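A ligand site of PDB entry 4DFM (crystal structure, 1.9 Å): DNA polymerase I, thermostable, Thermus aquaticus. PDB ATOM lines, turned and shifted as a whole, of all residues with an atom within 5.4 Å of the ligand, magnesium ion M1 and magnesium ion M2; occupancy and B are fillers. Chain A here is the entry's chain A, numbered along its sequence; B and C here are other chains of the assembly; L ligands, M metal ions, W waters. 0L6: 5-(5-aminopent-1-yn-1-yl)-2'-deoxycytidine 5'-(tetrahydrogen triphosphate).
Of the 25 residues printed, 3 come within 4 Å of magnesium ion M1.
Magnesium ion M1 is bound by O1B of the ligand (2.0 Å), O2G of the ligand (2.0 Å), O2A of the ligand (2.0 Å), OD2 of Asp 493 (2.0 Å), OD1 of Asp 318 (2.1 Å) and O of Tyr 319 (2.1 Å).
Magnesium ion M1 has six donor atoms within binding distance.
The side-chain amino group (NZ) of Lys 371 is in salt-bridge range of an oxygen (O1G) of the ligand, at 2.6 Å.
N1 of DG 4 of chain B lies within hydrogen-bond range of N3 of the ligand (2.8 Å).
NH1 of Arg 367 lies within salt-bridge range of O1G of the ligand (2.8 Å).
The backbone NH of Gln 321 sits at hydrogen-bond distance from an oxygen (O3G) of the ligand.
NE2 of His 347 is in hydrogen-bond range of O2B of the ligand (3.1 Å).
N of Glu 323 is in hydrogen-bond range of O3' of the ligand (3.2 Å).
The guanidinium group (NH2) of Arg 281 is in hydrogen-bond range of an oxygen (O4') of the ligand, at 3.3 Å.
The backbone NH (N) of Ile 322 lies close to an oxygen (O1B) of the ligand.
Water W6 binds magnesium ion M2, at 2.1 Å.
Water W4 binds magnesium ion M2, at 2.1 Å.
The side-chain carboxylate (OD2) of Asp 318 is bound to magnesium ion M2.
Magnesium ion M2 is bound by OD1 of Asp 493.
Magnesium ion M2 is bound by O2A of the ligand (2.4 Å).
Magnesium ion M2 has five donor atoms within binding distance.
OD2 of Asp 318 lies close to NZ of Lys 539 (3.3 Å).
OP2 of DDG 12 of chain C is in salt-bridge range of NH1 of Arg 368 (2.6 Å).
The guanidinium group (NH1) of Arg 281 lies within hydrogen-bond range of N3 of DDG 12 of chain C, at 3.0 Å.
N1 of DDG 12 of chain C sits close to N3 of DC 5 of chain B (2.5 Å).
NE2 of Gln 462 sits at hydrogen-bond distance from N2 of DDG 12 of chain C (3.2 Å).
The side-chain hydroxyl (OH) of Tyr 379 lies within hydrogen-bond range of the side-chain carboxylate (OE1) of Glu 323.
OP2 of DC 11 of chain C is in salt-bridge range of the guanidinium group (NH2) of Arg 368, at 3.95 Å.
O2 of DC 5 of chain B lies within hydrogen-bond range of NE2 of Gln 462, 3.4 Å away.
DDG 12 of chain C touches magnesium ion M2.
Within 4 Å of magnesium ion M2: Asp 318, Asp 493 and DDG 12 of chain C.
The nearest printed residue that does not touch magnesium ion M2 is Glu 494 (4.1 Å).
Merely in contact with the ligand: DDG 12 of chain C, Phe 375, Arg 368, Ser 320, Thr 372, DC 5 of chain B and DC 11 of chain C.
Hydrophobic or aromatic side chains within 4 Å of the ligand: Ile 322, His 347 and Phe 375.
Water W6 lies within hydrogen-bond range of the side-chain carboxylate (OE1) of Glu 494 (2.9 Å) and the backbone carbonyl oxygen (O) of Val 491 (3.0 Å).
Water W3 bridges N34 of the ligand (2.7 Å) and O6 of DDG 12 of chain C (2.8 Å).
Water W2 lies within hydrogen-bond range of NZ of Lys 371 and O1G of the ligand.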
ATOM      1  N   ARG A 281     -30.279  -6.695 -17.436  1.00  0.00           N
ATOM      2  CA  ARG A 281     -30.905  -7.658 -16.531  1.00  0.00           C
ATOM      3  C   ARG A 281     -31.882  -8.533 -17.321  1.00  0.00           C
ATOM      4  O   ARG A 281     -32.394  -8.125 -18.382  1.00  0.00           O
ATOM      5  CB  ARG A 281     -31.679  -6.953 -15.413  1.00  0.00           C
ATOM      6  CG  ARG A 281     -30.851  -6.503 -14.203  1.00  0.00           C
ATOM      7  CD  ARG A 281     -31.773  -6.049 -13.087  1.00  0.00           C
ATOM      8  NE  ARG A 281     -31.121  -5.914 -11.795  1.00  0.00           N
ATOM      9  CZ  ARG A 281     -31.774  -5.639 -10.672  1.00  0.00           C
ATOM     10  NH1 ARG A 281     -33.086  -5.457 -10.705  1.00  0.00           N
ATOM     11  NH2 ARG A 281     -31.118  -5.537  -9.526  1.00  0.00           N
ATOM     12  N   ASP A 318     -26.212 -16.229  -3.654  1.00  0.00           N
ATOM     13  CA  ASP A 318     -26.479 -14.797  -3.801  1.00  0.00           C
ATOM     14  C   ASP A 318     -25.177 -14.003  -3.664  1.00  0.00           C
ATOM     15  O   ASP A 318     -24.505 -14.100  -2.638  1.00  0.00           O
ATOM     16  CB  ASP A 318     -27.495 -14.370  -2.723  1.00  0.00           C
ATOM     17  CG  ASP A 318     -28.074 -12.967  -2.959  1.00  0.00           C
ATOM     18  OD1 ASP A 318     -27.280 -12.020  -3.174  1.00  0.00           O
ATOM     19  OD2 ASP A 318     -29.316 -12.813  -2.929  1.00  0.00           O
ATOM     20  N   TYR A 319     -24.826 -13.223  -4.688  1.00  0.00           N
ATOM     21  CA  TYR A 319     -23.645 -12.362  -4.615  1.00  0.00           C
ATOM     22  C   TYR A 319     -23.791 -11.325  -3.502  1.00  0.00           C
ATOM     23  O   TYR A 319     -24.826 -10.679  -3.387  1.00  0.00           O
ATOM     24  CB  TYR A 319     -23.389 -11.623  -5.934  1.00  0.00           C
ATOM     25  CG  TYR A 319     -22.765 -12.460  -7.025  1.00  0.00           C
ATOM     26  CD1 TYR A 319     -21.406 -12.754  -7.020  1.00  0.00           C
ATOM     27  CD2 TYR A 319     -23.524 -12.911  -8.092  1.00  0.00           C
ATOM     28  CE1 TYR A 319     -20.831 -13.510  -8.028  1.00  0.00           C
ATOM     29  CE2 TYR A 319     -22.960 -13.662  -9.111  1.00  0.00           C
ATOM     30  CZ  TYR A 319     -21.609 -13.965  -9.069  1.00  0.00           C
ATOM     31  OH  TYR A 319     -21.053 -14.711 -10.078  1.00  0.00           O
ATOM     32  N   SER A 320     -22.744 -11.187  -2.701  1.00  0.00           N
ATOM     33  CA  SER A 320     -22.740 -10.241  -1.587  1.00  0.00           C
ATOM     34  C   SER A 320     -22.439  -8.810  -2.048  1.00  0.00           C
ATOM     35  O   SER A 320     -21.459  -8.585  -2.760  1.00  0.00           O
ATOM     36  CB  SER A 320     -21.715 -10.691  -0.536  1.00  0.00           C
ATOM     37  OG  SER A 320     -21.276  -9.608   0.267  1.00  0.00           O
ATOM     38  N   GLN A 321     -23.296  -7.855  -1.656  1.00  0.00           N
ATOM     39  CA  GLN A 321     -23.088  -6.433  -1.929  1.00  0.00           C
ATOM     40  C   GLN A 321     -22.657  -6.185  -3.374  1.00  0.00           C
ATOM     41  O   GLN A 321     -21.738  -5.405  -3.624  1.00  0.00           O
ATOM     42  CB  GLN A 321     -22.043  -5.857  -0.966  1.00  0.00           C
ATOM     43  CG  GLN A 321     -22.203  -6.297   0.503  1.00  0.00           C
ATOM     44  CD  GLN A 321     -21.125  -5.741   1.416  1.00  0.00           C
ATOM     45  OE1 GLN A 321     -21.059  -4.538   1.647  1.00  0.00           O
ATOM     46  NE2 GLN A 321     -20.261  -6.613   1.923  1.00  0.00           N
ATOM     47  N   ILE A 322     -23.308  -6.854  -4.312  1.00  0.00           N
ATOM     48  CA  ILE A 322     -22.767  -6.953  -5.671  1.00  0.00           C
ATOM     49  C   ILE A 322     -22.549  -5.620  -6.396  1.00  0.00           C
ATOM     50  O   ILE A 322     -21.484  -5.383  -6.960  1.00  0.00           O
ATOM     51  CB  ILE A 322     -23.556  -7.958  -6.556  1.00  0.00           C
ATOM     52  CG1 ILE A 322     -22.838  -8.167  -7.890  1.00  0.00           C
ATOM     53  CG2 ILE A 322     -24.992  -7.502  -6.770  1.00  0.00           C
ATOM     54  CD1 ILE A 322     -21.404  -8.654  -7.748  1.00  0.00           C
ATOM     55  N   GLU A 323     -23.531  -4.731  -6.377  1.00  0.00           N
ATOM     56  CA  GLU A 323     -23.360  -3.479  -7.102  1.00  0.00           C
ATOM     57  C   GLU A 323     -22.305  -2.572  -6.466  1.00  0.00           C
ATOM     58  O   GLU A 323     -21.645  -1.800  -7.168  1.00  0.00           O
ATOM     59  CB  GLU A 323     -24.698  -2.782  -7.329  1.00  0.00           C
ATOM     60  CG  GLU A 323     -25.555  -3.527  -8.355  1.00  0.00           C
ATOM     61  CD  GLU A 323     -26.774  -2.738  -8.816  1.00  0.00           C
ATOM     62  OE1 GLU A 323     -26.777  -1.503  -8.656  1.00  0.00           O
ATOM     63  OE2 GLU A 323     -27.715  -3.355  -9.333  1.00  0.00           O
ATOM     64  N   LEU A 324     -22.125  -2.673  -5.151  1.00  0.00           N
ATOM     65  CA  LEU A 324     -21.097  -1.887  -4.467  1.00  0.00           C
ATOM     66  C   LEU A 324     -19.705  -2.378  -4.884  1.00  0.00           C
ATOM     67  O   LEU A 324     -18.816  -1.582  -5.147  1.00  0.00           O
ATOM     68  CB  LEU A 324     -21.239  -1.952  -2.943  1.00  0.00           C
ATOM     69  CG  LEU A 324     -22.427  -1.267  -2.251  1.00  0.00           C
ATOM     70  CD1 LEU A 324     -22.258  -1.284  -0.728  1.00  0.00           C
ATOM     71  CD2 LEU A 324     -22.625   0.159  -2.753  1.00  0.00           C
ATOM     72  N   HIS A 347     -23.615  -2.630   4.211  1.00  0.00           N
ATOM     73  CA  HIS A 347     -25.018  -2.744   4.590  1.00  0.00           C
ATOM     74  C   HIS A 347     -25.171  -2.864   6.109  1.00  0.00           C
ATOM     75  O   HIS A 347     -26.024  -2.205   6.701  1.00  0.00           O
ATOM     76  CB  HIS A 347     -25.667  -3.936   3.891  1.00  0.00           C
ATOM     77  CG  HIS A 347     -25.752  -3.802   2.406  1.00  0.00           C
ATOM     78  ND1 HIS A 347     -25.904  -2.578   1.779  1.00  0.00           N
ATOM     79  CD2 HIS A 347     -25.682  -4.719   1.411  1.00  0.00           C
ATOM     80  CE1 HIS A 347     -25.939  -2.756   0.470  1.00  0.00           C
ATOM     81  NE2 HIS A 347     -25.801  -4.047   0.222  1.00  0.00           N
ATOM     82  N   ARG A 367     -30.546  -5.000   8.391  1.00  0.00           N
ATOM     83  CA  ARG A 367     -29.605  -4.937   7.281  1.00  0.00           C
ATOM     84  C   ARG A 367     -30.332  -4.719   5.965  1.00  0.00           C
ATOM     85  O   ARG A 367     -29.899  -3.911   5.137  1.00  0.00           O
ATOM     86  CB  ARG A 367     -28.779  -6.215   7.224  1.00  0.00           C
ATOM     87  CG  ARG A 367     -27.645  -6.161   6.219  1.00  0.00           C
ATOM     88  CD  ARG A 367     -26.780  -7.400   6.319  1.00  0.00           C
ATOM     89  NE  ARG A 367     -25.748  -7.403   5.286  1.00  0.00           N
ATOM     90  CZ  ARG A 367     -25.958  -7.782   4.025  1.00  0.00           C
ATOM     91  NH1 ARG A 367     -27.162  -8.179   3.640  1.00  0.00           N
ATOM     92  NH2 ARG A 367     -24.965  -7.754   3.161  1.00  0.00           N
ATOM     93  N   ARG A 368     -31.437  -5.431   5.768  1.00  0.00           N
ATOM     94  CA  ARG A 368     -32.260  -5.291   4.570  1.00  0.00           C
ATOM     95  C   ARG A 368     -32.760  -3.851   4.424  1.00  0.00           C
ATOM     96  O   ARG A 368     -32.767  -3.305   3.324  1.00  0.00           O
ATOM     97  CB  ARG A 368     -33.442  -6.259   4.585  1.00  0.00           C
ATOM     98  CG  ARG A 368     -34.416  -6.069   3.429  1.00  0.00           C
ATOM     99  CD  ARG A 368     -35.634  -6.964   3.571  1.00  0.00           C
ATOM    100  NE  ARG A 368     -36.594  -6.783   2.489  1.00  0.00           N
ATOM    101  CZ  ARG A 368     -36.521  -7.387   1.309  1.00  0.00           C
ATOM    102  NH1 ARG A 368     -35.519  -8.229   1.064  1.00  0.00           N
ATOM    103  NH2 ARG A 368     -37.439  -7.165   0.374  1.00  0.00           N
ATOM    104  N   LYS A 371     -30.100  -1.711   3.075  1.00  0.00           N
ATOM    105  CA  LYS A 371     -29.803  -1.904   1.659  1.00  0.00           C
ATOM    106  C   LYS A 371     -30.463  -0.834   0.815  1.00  0.00           C
ATOM    107  O   LYS A 371     -29.837  -0.229  -0.063  1.00  0.00           O
ATOM    108  CB  LYS A 371     -30.282  -3.264   1.167  1.00  0.00           C
ATOM    109  CG  LYS A 371     -29.429  -4.429   1.589  1.00  0.00           C
ATOM    110  CD  LYS A 371     -29.671  -5.595   0.651  1.00  0.00           C
ATOM    111  CE  LYS A 371     -29.718  -6.897   1.402  1.00  0.00           C
ATOM    112  NZ  LYS A 371     -29.869  -8.049   0.468  1.00  0.00           N
ATOM    113  N   THR A 372     -31.744  -0.607   1.075  1.00  0.00           N
ATOM    114  CA  THR A 372     -32.512   0.391   0.336  1.00  0.00           C
ATOM    115  C   THR A 372     -31.886   1.771   0.518  1.00  0.00           C
ATOM    116  O   THR A 372     -31.771   2.537  -0.426  1.00  0.00           O
ATOM    117  CB  THR A 372     -33.988   0.391   0.770  1.00  0.00           C
ATOM    118  OG1 THR A 372     -34.568  -0.884   0.456  1.00  0.00           O
ATOM    119  CG2 THR A 372     -34.762   1.491   0.065  1.00  0.00           C
ATOM    120  N   PHE A 375     -28.315   1.924  -1.469  1.00  0.00           N
ATOM    121  CA  PHE A 375     -28.474   2.087  -2.911  1.00  0.00           C
ATOM    122  C   PHE A 375     -29.300   3.329  -3.275  1.00  0.00           C
ATOM    123  O   PHE A 375     -29.028   3.990  -4.282  1.00  0.00           O
ATOM    124  CB  PHE A 375     -29.061   0.824  -3.550  1.00  0.00           C
ATOM    125  CG  PHE A 375     -28.173  -0.381  -3.374  1.00  0.00           C
ATOM    126  CD1 PHE A 375     -26.879  -0.370  -3.878  1.00  0.00           C
ATOM    127  CD2 PHE A 375     -28.615  -1.490  -2.686  1.00  0.00           C
ATOM    128  CE1 PHE A 375     -26.047  -1.467  -3.709  1.00  0.00           C
ATOM    129  CE2 PHE A 375     -27.778  -2.595  -2.517  1.00  0.00           C
ATOM    130  CZ  PHE A 375     -26.496  -2.568  -3.020  1.00  0.00           C
ATOM    131  N   TYR A 379     -27.716   6.195  -5.723  1.00  0.00           N
ATOM    132  CA  TYR A 379     -28.312   6.539  -7.008  1.00  0.00           C
ATOM    133  C   TYR A 379     -29.195   7.792  -6.992  1.00  0.00           C
ATOM    134  O   TYR A 379     -30.026   7.984  -7.873  1.00  0.00           O
ATOM    135  CB  TYR A 379     -29.051   5.334  -7.584  1.00  0.00           C
ATOM    136  CG  TYR A 379     -28.130   4.167  -7.844  1.00  0.00           C
ATOM    137  CD1 TYR A 379     -27.131   4.244  -8.801  1.00  0.00           C
ATOM    138  CD2 TYR A 379     -28.248   2.989  -7.121  1.00  0.00           C
ATOM    139  CE1 TYR A 379     -26.276   3.188  -9.049  1.00  0.00           C
ATOM    140  CE2 TYR A 379     -27.392   1.920  -7.350  1.00  0.00           C
ATOM    141  CZ  TYR A 379     -26.417   2.018  -8.317  1.00  0.00           C
ATOM    142  OH  TYR A 379     -25.562   0.962  -8.565  1.00  0.00           O
ATOM    143  N   ASN A 458     -26.495   4.688 -13.306  1.00  0.00           N
ATOM    144  CA  ASN A 458     -26.882   3.418 -12.709  1.00  0.00           C
ATOM    145  C   ASN A 458     -26.597   2.255 -13.641  1.00  0.00           C
ATOM    146  O   ASN A 458     -26.142   1.199 -13.199  1.00  0.00           O
ATOM    147  CB  ASN A 458     -28.370   3.428 -12.328  1.00  0.00           C
ATOM    148  CG  ASN A 458     -28.887   2.050 -11.956  1.00  0.00           C
ATOM    149  OD1 ASN A 458     -29.405   1.320 -12.806  1.00  0.00           O
ATOM    150  ND2 ASN A 458     -28.738   1.687 -10.693  1.00  0.00           N
ATOM    151  N   GLN A 462     -25.532  -1.629 -12.552  1.00  0.00           N
ATOM    152  CA  GLN A 462     -26.532  -2.697 -12.604  1.00  0.00           C
ATOM    153  C   GLN A 462     -26.254  -3.636 -13.768  1.00  0.00           C
ATOM    154  O   GLN A 462     -26.325  -4.863 -13.626  1.00  0.00           O
ATOM    155  CB  GLN A 462     -27.953  -2.118 -12.710  1.00  0.00           C
ATOM    156  CG  GLN A 462     -29.044  -3.184 -12.666  1.00  0.00           C
ATOM    157  CD  GLN A 462     -30.436  -2.614 -12.863  1.00  0.00           C
ATOM    158  OE1 GLN A 462     -31.081  -2.879 -13.889  1.00  0.00           O
ATOM    159  NE2 GLN A 462     -30.914  -1.848 -11.894  1.00  0.00           N
ATOM    160  N   VAL A 491     -32.607 -14.672  -9.878  1.00  0.00           N
ATOM    161  CA  VAL A 491     -33.243 -13.447  -9.379  1.00  0.00           C
ATOM    162  C   VAL A 491     -32.182 -12.355  -9.265  1.00  0.00           C
ATOM    163  O   VAL A 491     -31.788 -11.942  -8.175  1.00  0.00           O
ATOM    164  CB  VAL A 491     -33.954 -13.665  -8.013  1.00  0.00           C
ATOM    165  CG1 VAL A 491     -34.776 -12.414  -7.634  1.00  0.00           C
ATOM    166  CG2 VAL A 491     -34.859 -14.885  -8.081  1.00  0.00           C
ATOM    167  N   ASP A 493     -29.116 -11.253  -8.828  1.00  0.00           N
ATOM    168  CA  ASP A 493     -27.787 -11.621  -8.363  1.00  0.00           C
ATOM    169  C   ASP A 493     -27.846 -12.900  -7.556  1.00  0.00           C
ATOM    170  O   ASP A 493     -26.933 -13.209  -6.781  1.00  0.00           O
ATOM    171  CB  ASP A 493     -27.137 -10.486  -7.572  1.00  0.00           C
ATOM    172  CG  ASP A 493     -27.645 -10.394  -6.156  1.00  0.00           C
ATOM    173  OD1 ASP A 493     -28.856 -10.617  -5.918  1.00  0.00           O
ATOM    174  OD2 ASP A 493     -26.816 -10.098  -5.259  1.00  0.00           O
ATOM    175  N   GLU A 494     -28.914 -13.658  -7.768  1.00  0.00           N
ATOM    176  CA  GLU A 494     -29.156 -14.887  -7.032  1.00  0.00           C
ATOM    177  C   GLU A 494     -29.487 -16.014  -8.002  1.00  0.00           C
ATOM    178  O   GLU A 494     -30.167 -15.802  -9.012  1.00  0.00           O
ATOM    179  CB  GLU A 494     -30.320 -14.689  -6.055  1.00  0.00           C
ATOM    180  CG  GLU A 494     -30.797 -15.957  -5.362  1.00  0.00           C
ATOM    181  CD  GLU A 494     -32.002 -15.708  -4.467  1.00  0.00           C
ATOM    182  OE1 GLU A 494     -32.435 -14.539  -4.358  1.00  0.00           O
ATOM    183  OE2 GLU A 494     -32.503 -16.679  -3.863  1.00  0.00           O
ATOM    184  N   LYS A 539     -32.274 -19.811   2.006  1.00  0.00           N
ATOM    185  CA  LYS A 539     -31.633 -18.495   2.069  1.00  0.00           C
ATOM    186  C   LYS A 539     -31.151 -18.134   3.473  1.00  0.00           C
ATOM    187  O   LYS A 539     -30.488 -17.120   3.666  1.00  0.00           O
ATOM    188  CB  LYS A 539     -32.553 -17.390   1.533  1.00  0.00           C
ATOM    189  CG  LYS A 539     -32.904 -17.532   0.066  1.00  0.00           C
ATOM    190  CD  LYS A 539     -33.146 -16.171  -0.599  1.00  0.00           C
ATOM    191  CE  LYS A 539     -31.834 -15.404  -0.763  1.00  0.00           C
ATOM    192  NZ  LYS A 539     -32.025 -14.082  -1.426  1.00  0.00           N
ATOM    193  P    DG B   4     -36.303  10.467  -4.685  1.00  0.00           P
ATOM    194  OP1  DG B   4     -37.576   9.756  -4.425  1.00  0.00           O
ATOM    195  OP2  DG B   4     -35.711  11.330  -3.638  1.00  0.00           O
ATOM    196  O5'  DG B   4     -35.171   9.401  -5.105  1.00  0.00           O
ATOM    197  C5'  DG B   4     -35.347   8.607  -6.262  1.00  0.00           C
ATOM    198  C4'  DG B   4     -33.993   8.120  -6.750  1.00  0.00           C
ATOM    199  O4'  DG B   4     -33.253   7.538  -5.649  1.00  0.00           O
ATOM    200  C3'  DG B   4     -34.070   7.059  -7.835  1.00  0.00           C
ATOM    201  O3'  DG B   4     -34.007   7.716  -9.071  1.00  0.00           O
ATOM    202  C2'  DG B   4     -32.797   6.242  -7.590  1.00  0.00           C
ATOM    203  C1'  DG B   4     -32.626   6.337  -6.070  1.00  0.00           C
ATOM    204  N9   DG B   4     -33.224   5.236  -5.320  1.00  0.00           N
ATOM    205  C8   DG B   4     -34.217   5.322  -4.364  1.00  0.00           C
ATOM    206  N7   DG B   4     -34.530   4.161  -3.850  1.00  0.00           N
ATOM    207  C5   DG B   4     -33.703   3.257  -4.509  1.00  0.00           C
ATOM    208  C6   DG B   4     -33.602   1.857  -4.382  1.00  0.00           C
ATOM    209  O6   DG B   4     -34.243   1.118  -3.626  1.00  0.00           O
ATOM    210  N1   DG B   4     -32.633   1.328  -5.233  1.00  0.00           N
ATOM    211  C2   DG B   4     -31.871   2.053  -6.113  1.00  0.00           C
ATOM    212  N2   DG B   4     -30.997   1.362  -6.867  1.00  0.00           N
ATOM    213  N3   DG B   4     -31.965   3.372  -6.248  1.00  0.00           N
ATOM    214  C4   DG B   4     -32.893   3.908  -5.418  1.00  0.00           C
ATOM    215  P    DC B   5     -34.945   7.262 -10.286  1.00  0.00           P
ATOM    216  OP1  DC B   5     -34.857   8.300 -11.336  1.00  0.00           O
ATOM    217  OP2  DC B   5     -36.263   6.873  -9.723  1.00  0.00           O
ATOM    218  O5'  DC B   5     -34.232   5.938 -10.844  1.00  0.00           O
ATOM    219  C5'  DC B   5     -32.945   6.040 -11.453  1.00  0.00           C
ATOM    220  C4'  DC B   5     -32.330   4.661 -11.636  1.00  0.00           C
ATOM    221  O4'  DC B   5     -32.114   4.060 -10.333  1.00  0.00           O
ATOM    222  C3'  DC B   5     -33.214   3.650 -12.365  1.00  0.00           C
ATOM    223  O3'  DC B   5     -33.099   3.747 -13.782  1.00  0.00           O
ATOM    224  C2'  DC B   5     -32.610   2.328 -11.882  1.00  0.00           C
ATOM    225  C1'  DC B   5     -32.293   2.654 -10.419  1.00  0.00           C
ATOM    226  N1   DC B   5     -33.326   2.205  -9.416  1.00  0.00           N
ATOM    227  C2   DC B   5     -33.407   0.855  -9.075  1.00  0.00           C
ATOM    228  O2   DC B   5     -32.646   0.042  -9.621  1.00  0.00           O
ATOM    229  N3   DC B   5     -34.318   0.463  -8.156  1.00  0.00           N
ATOM    230  C4   DC B   5     -35.130   1.361  -7.589  1.00  0.00           C
ATOM    231  N4   DC B   5     -36.019   0.925  -6.687  1.00  0.00           N
ATOM    232  C5   DC B   5     -35.059   2.741  -7.925  1.00  0.00           C
ATOM    233  C6   DC B   5     -34.152   3.118  -8.838  1.00  0.00           C
ATOM    234  P    DC C  11     -41.277  -8.140  -0.989  1.00  0.00           P
ATOM    235  OP1  DC C  11     -41.098  -9.173   0.050  1.00  0.00           O
ATOM    236  OP2  DC C  11     -41.240  -6.712  -0.613  1.00  0.00           O
ATOM    237  O5'  DC C  11     -40.171  -8.338  -2.137  1.00  0.00           O
ATOM    238  C5'  DC C  11     -40.035  -9.627  -2.702  1.00  0.00           C
ATOM    239  C4'  DC C  11     -39.182  -9.625  -3.964  1.00  0.00           C
ATOM    240  O4'  DC C  11     -39.793  -8.753  -4.952  1.00  0.00           O
ATOM    241  C3'  DC C  11     -37.758  -9.114  -3.817  1.00  0.00           C
ATOM    242  O3'  DC C  11     -36.910 -10.167  -3.317  1.00  0.00           O
ATOM    243  C2'  DC C  11     -37.443  -8.763  -5.273  1.00  0.00           C
ATOM    244  C1'  DC C  11     -38.778  -8.210  -5.778  1.00  0.00           C
ATOM    245  N1   DC C  11     -38.888  -6.736  -5.720  1.00  0.00           N
ATOM    246  C2   DC C  11     -38.403  -6.003  -6.809  1.00  0.00           C
ATOM    247  O2   DC C  11     -37.907  -6.625  -7.748  1.00  0.00           O
ATOM    248  N3   DC C  11     -38.514  -4.636  -6.788  1.00  0.00           N
ATOM    249  C4   DC C  11     -39.069  -4.029  -5.739  1.00  0.00           C
ATOM    250  N4   DC C  11     -39.157  -2.691  -5.763  1.00  0.00           N
ATOM    251  C5   DC C  11     -39.567  -4.761  -4.621  1.00  0.00           C
ATOM    252  C6   DC C  11     -39.462  -6.107  -4.659  1.00  0.00           C
ATOM    253  P   DDG C  12     -35.528  -9.616  -2.716  1.00  0.00           P
ATOM    254  OP1 DDG C  12     -35.395 -11.054  -2.316  1.00  0.00           O
ATOM    255  OP2 DDG C  12     -35.789  -8.767  -1.507  1.00  0.00           O
ATOM    256  O5' DDG C  12     -34.594  -9.054  -3.850  1.00  0.00           O
ATOM    257  C5' DDG C  12     -34.147  -9.925  -4.853  1.00  0.00           C
ATOM    258  C4' DDG C  12     -33.411  -9.092  -5.912  1.00  0.00           C
ATOM    259  O4' DDG C  12     -34.277  -8.223  -6.537  1.00  0.00           O
ATOM    260  C3' DDG C  12     -32.312  -8.249  -5.313  1.00  0.00           C
ATOM    261  C2' DDG C  12     -32.165  -7.235  -6.441  1.00  0.00           C
ATOM    262  C1' DDG C  12     -33.581  -7.122  -6.926  1.00  0.00           C
ATOM    263  N9  DDG C  12     -34.211  -5.960  -6.368  1.00  0.00           N
ATOM    264  C8  DDG C  12     -35.006  -5.934  -5.234  1.00  0.00           C
ATOM    265  N7  DDG C  12     -35.438  -4.639  -5.020  1.00  0.00           N
ATOM    266  C5  DDG C  12     -34.888  -3.866  -6.053  1.00  0.00           C
ATOM    267  C6  DDG C  12     -34.972  -2.448  -6.383  1.00  0.00           C
ATOM    268  O6  DDG C  12     -35.713  -1.632  -5.567  1.00  0.00           O
ATOM    269  N1  DDG C  12     -34.314  -1.960  -7.494  1.00  0.00           N
ATOM    270  C2  DDG C  12     -33.548  -2.832  -8.307  1.00  0.00           C
ATOM    271  N2  DDG C  12     -32.880  -2.321  -9.452  1.00  0.00           N
ATOM    272  N3  DDG C  12     -33.473  -4.178  -8.014  1.00  0.00           N
ATOM    273  C4  DDG C  12     -34.129  -4.691  -6.898  1.00  0.00           C
HETATM  274  O2  0L6 L   1     -30.543  -1.302  -6.679  1.00  0.00           O
HETATM  275  C2  0L6 L   1     -30.997  -1.942  -5.697  1.00  0.00           C
HETATM  276  N3  0L6 L   1     -31.861  -1.375  -4.855  1.00  0.00           N
HETATM  277  C4  0L6 L   1     -32.348  -2.056  -3.817  1.00  0.00           C
HETATM  278  N4  0L6 L   1     -33.230  -1.464  -2.973  1.00  0.00           N
HETATM  279  C5  0L6 L   1     -31.979  -3.348  -3.591  1.00  0.00           C
HETATM  280  C29 0L6 L   1     -32.501  -3.941  -2.581  1.00  0.00           C
HETATM  281  C30 0L6 L   1     -32.984  -4.486  -1.655  1.00  0.00           C
HETATM  282  C31 0L6 L   1     -33.552  -5.128  -0.446  1.00  0.00           C
HETATM  283  C32 0L6 L   1     -35.041  -4.749  -0.364  1.00  0.00           C
HETATM  284  C33 0L6 L   1     -35.783  -5.158  -1.639  1.00  0.00           C
HETATM  285  N34 0L6 L   1     -36.908  -4.275  -1.855  1.00  0.00           N
HETATM  286  C6  0L6 L   1     -31.074  -3.995  -4.464  1.00  0.00           C
HETATM  287  N1  0L6 L   1     -30.596  -3.284  -5.497  1.00  0.00           N
HETATM  288  C1' 0L6 L   1     -29.628  -3.867  -6.446  1.00  0.00           C
HETATM  289  O4' 0L6 L   1     -29.735  -5.298  -6.511  1.00  0.00           O
HETATM  290  C2' 0L6 L   1     -28.252  -3.550  -5.883  1.00  0.00           C
HETATM  291  C3' 0L6 L   1     -27.863  -4.856  -5.202  1.00  0.00           C
HETATM  292  O3' 0L6 L   1     -26.447  -4.998  -5.083  1.00  0.00           O
HETATM  293  C4' 0L6 L   1     -28.496  -5.896  -6.103  1.00  0.00           C
HETATM  294  C5' 0L6 L   1     -28.704  -7.256  -5.423  1.00  0.00           C
HETATM  295  O5' 0L6 L   1     -29.602  -7.127  -4.330  1.00  0.00           O
HETATM  296  PA  0L6 L   1     -29.316  -7.942  -2.969  1.00  0.00           P
HETATM  297  O1A 0L6 L   1     -30.585  -7.927  -2.157  1.00  0.00           O
HETATM  298  O2A 0L6 L   1     -28.647  -9.273  -3.244  1.00  0.00           O
HETATM  299  O3A 0L6 L   1     -28.299  -6.884  -2.272  1.00  0.00           O
HETATM  300  PB  0L6 L   1     -26.698  -7.036  -2.219  1.00  0.00           P
HETATM  301  O1B 0L6 L   1     -26.222  -8.113  -3.171  1.00  0.00           O
HETATM  302  O2B 0L6 L   1     -26.131  -5.641  -2.395  1.00  0.00           O
HETATM  303  O3B 0L6 L   1     -26.439  -7.434  -0.665  1.00  0.00           O
HETATM  304  PG  0L6 L   1     -26.368  -8.932  -0.072  1.00  0.00           P
HETATM  305  O1G 0L6 L   1     -27.472  -8.956   0.968  1.00  0.00           O
HETATM  306  O2G 0L6 L   1     -26.613  -9.859  -1.247  1.00  0.00           O
HETATM  307  O3G 0L6 L   1     -24.993  -9.025   0.546  1.00  0.00           O
HETATM  308 MG    MG M   1     -26.787 -10.002  -3.222  1.00  0.00          MG
HETATM  309 MG    MG M   2     -30.026 -11.093  -4.045  1.00  0.00          MG
HETATM  310  O   HOH W   1     -25.526 -12.371  -0.517  1.00  0.00           O
HETATM  311  O   HOH W   2     -29.475 -10.914  -0.454  1.00  0.00           O
HETATM  312  O   HOH W   3     -36.974  -1.920  -3.077  1.00  0.00           O
HETATM  313  O   HOH W   4     -31.291 -10.610  -2.397  1.00  0.00           O
HETATM  314  O   HOH W   5     -29.457  -0.958  -9.396  1.00  0.00           O
HETATM  315  O   HOH W   6     -31.572 -11.908  -5.193  1.00  0.00           O
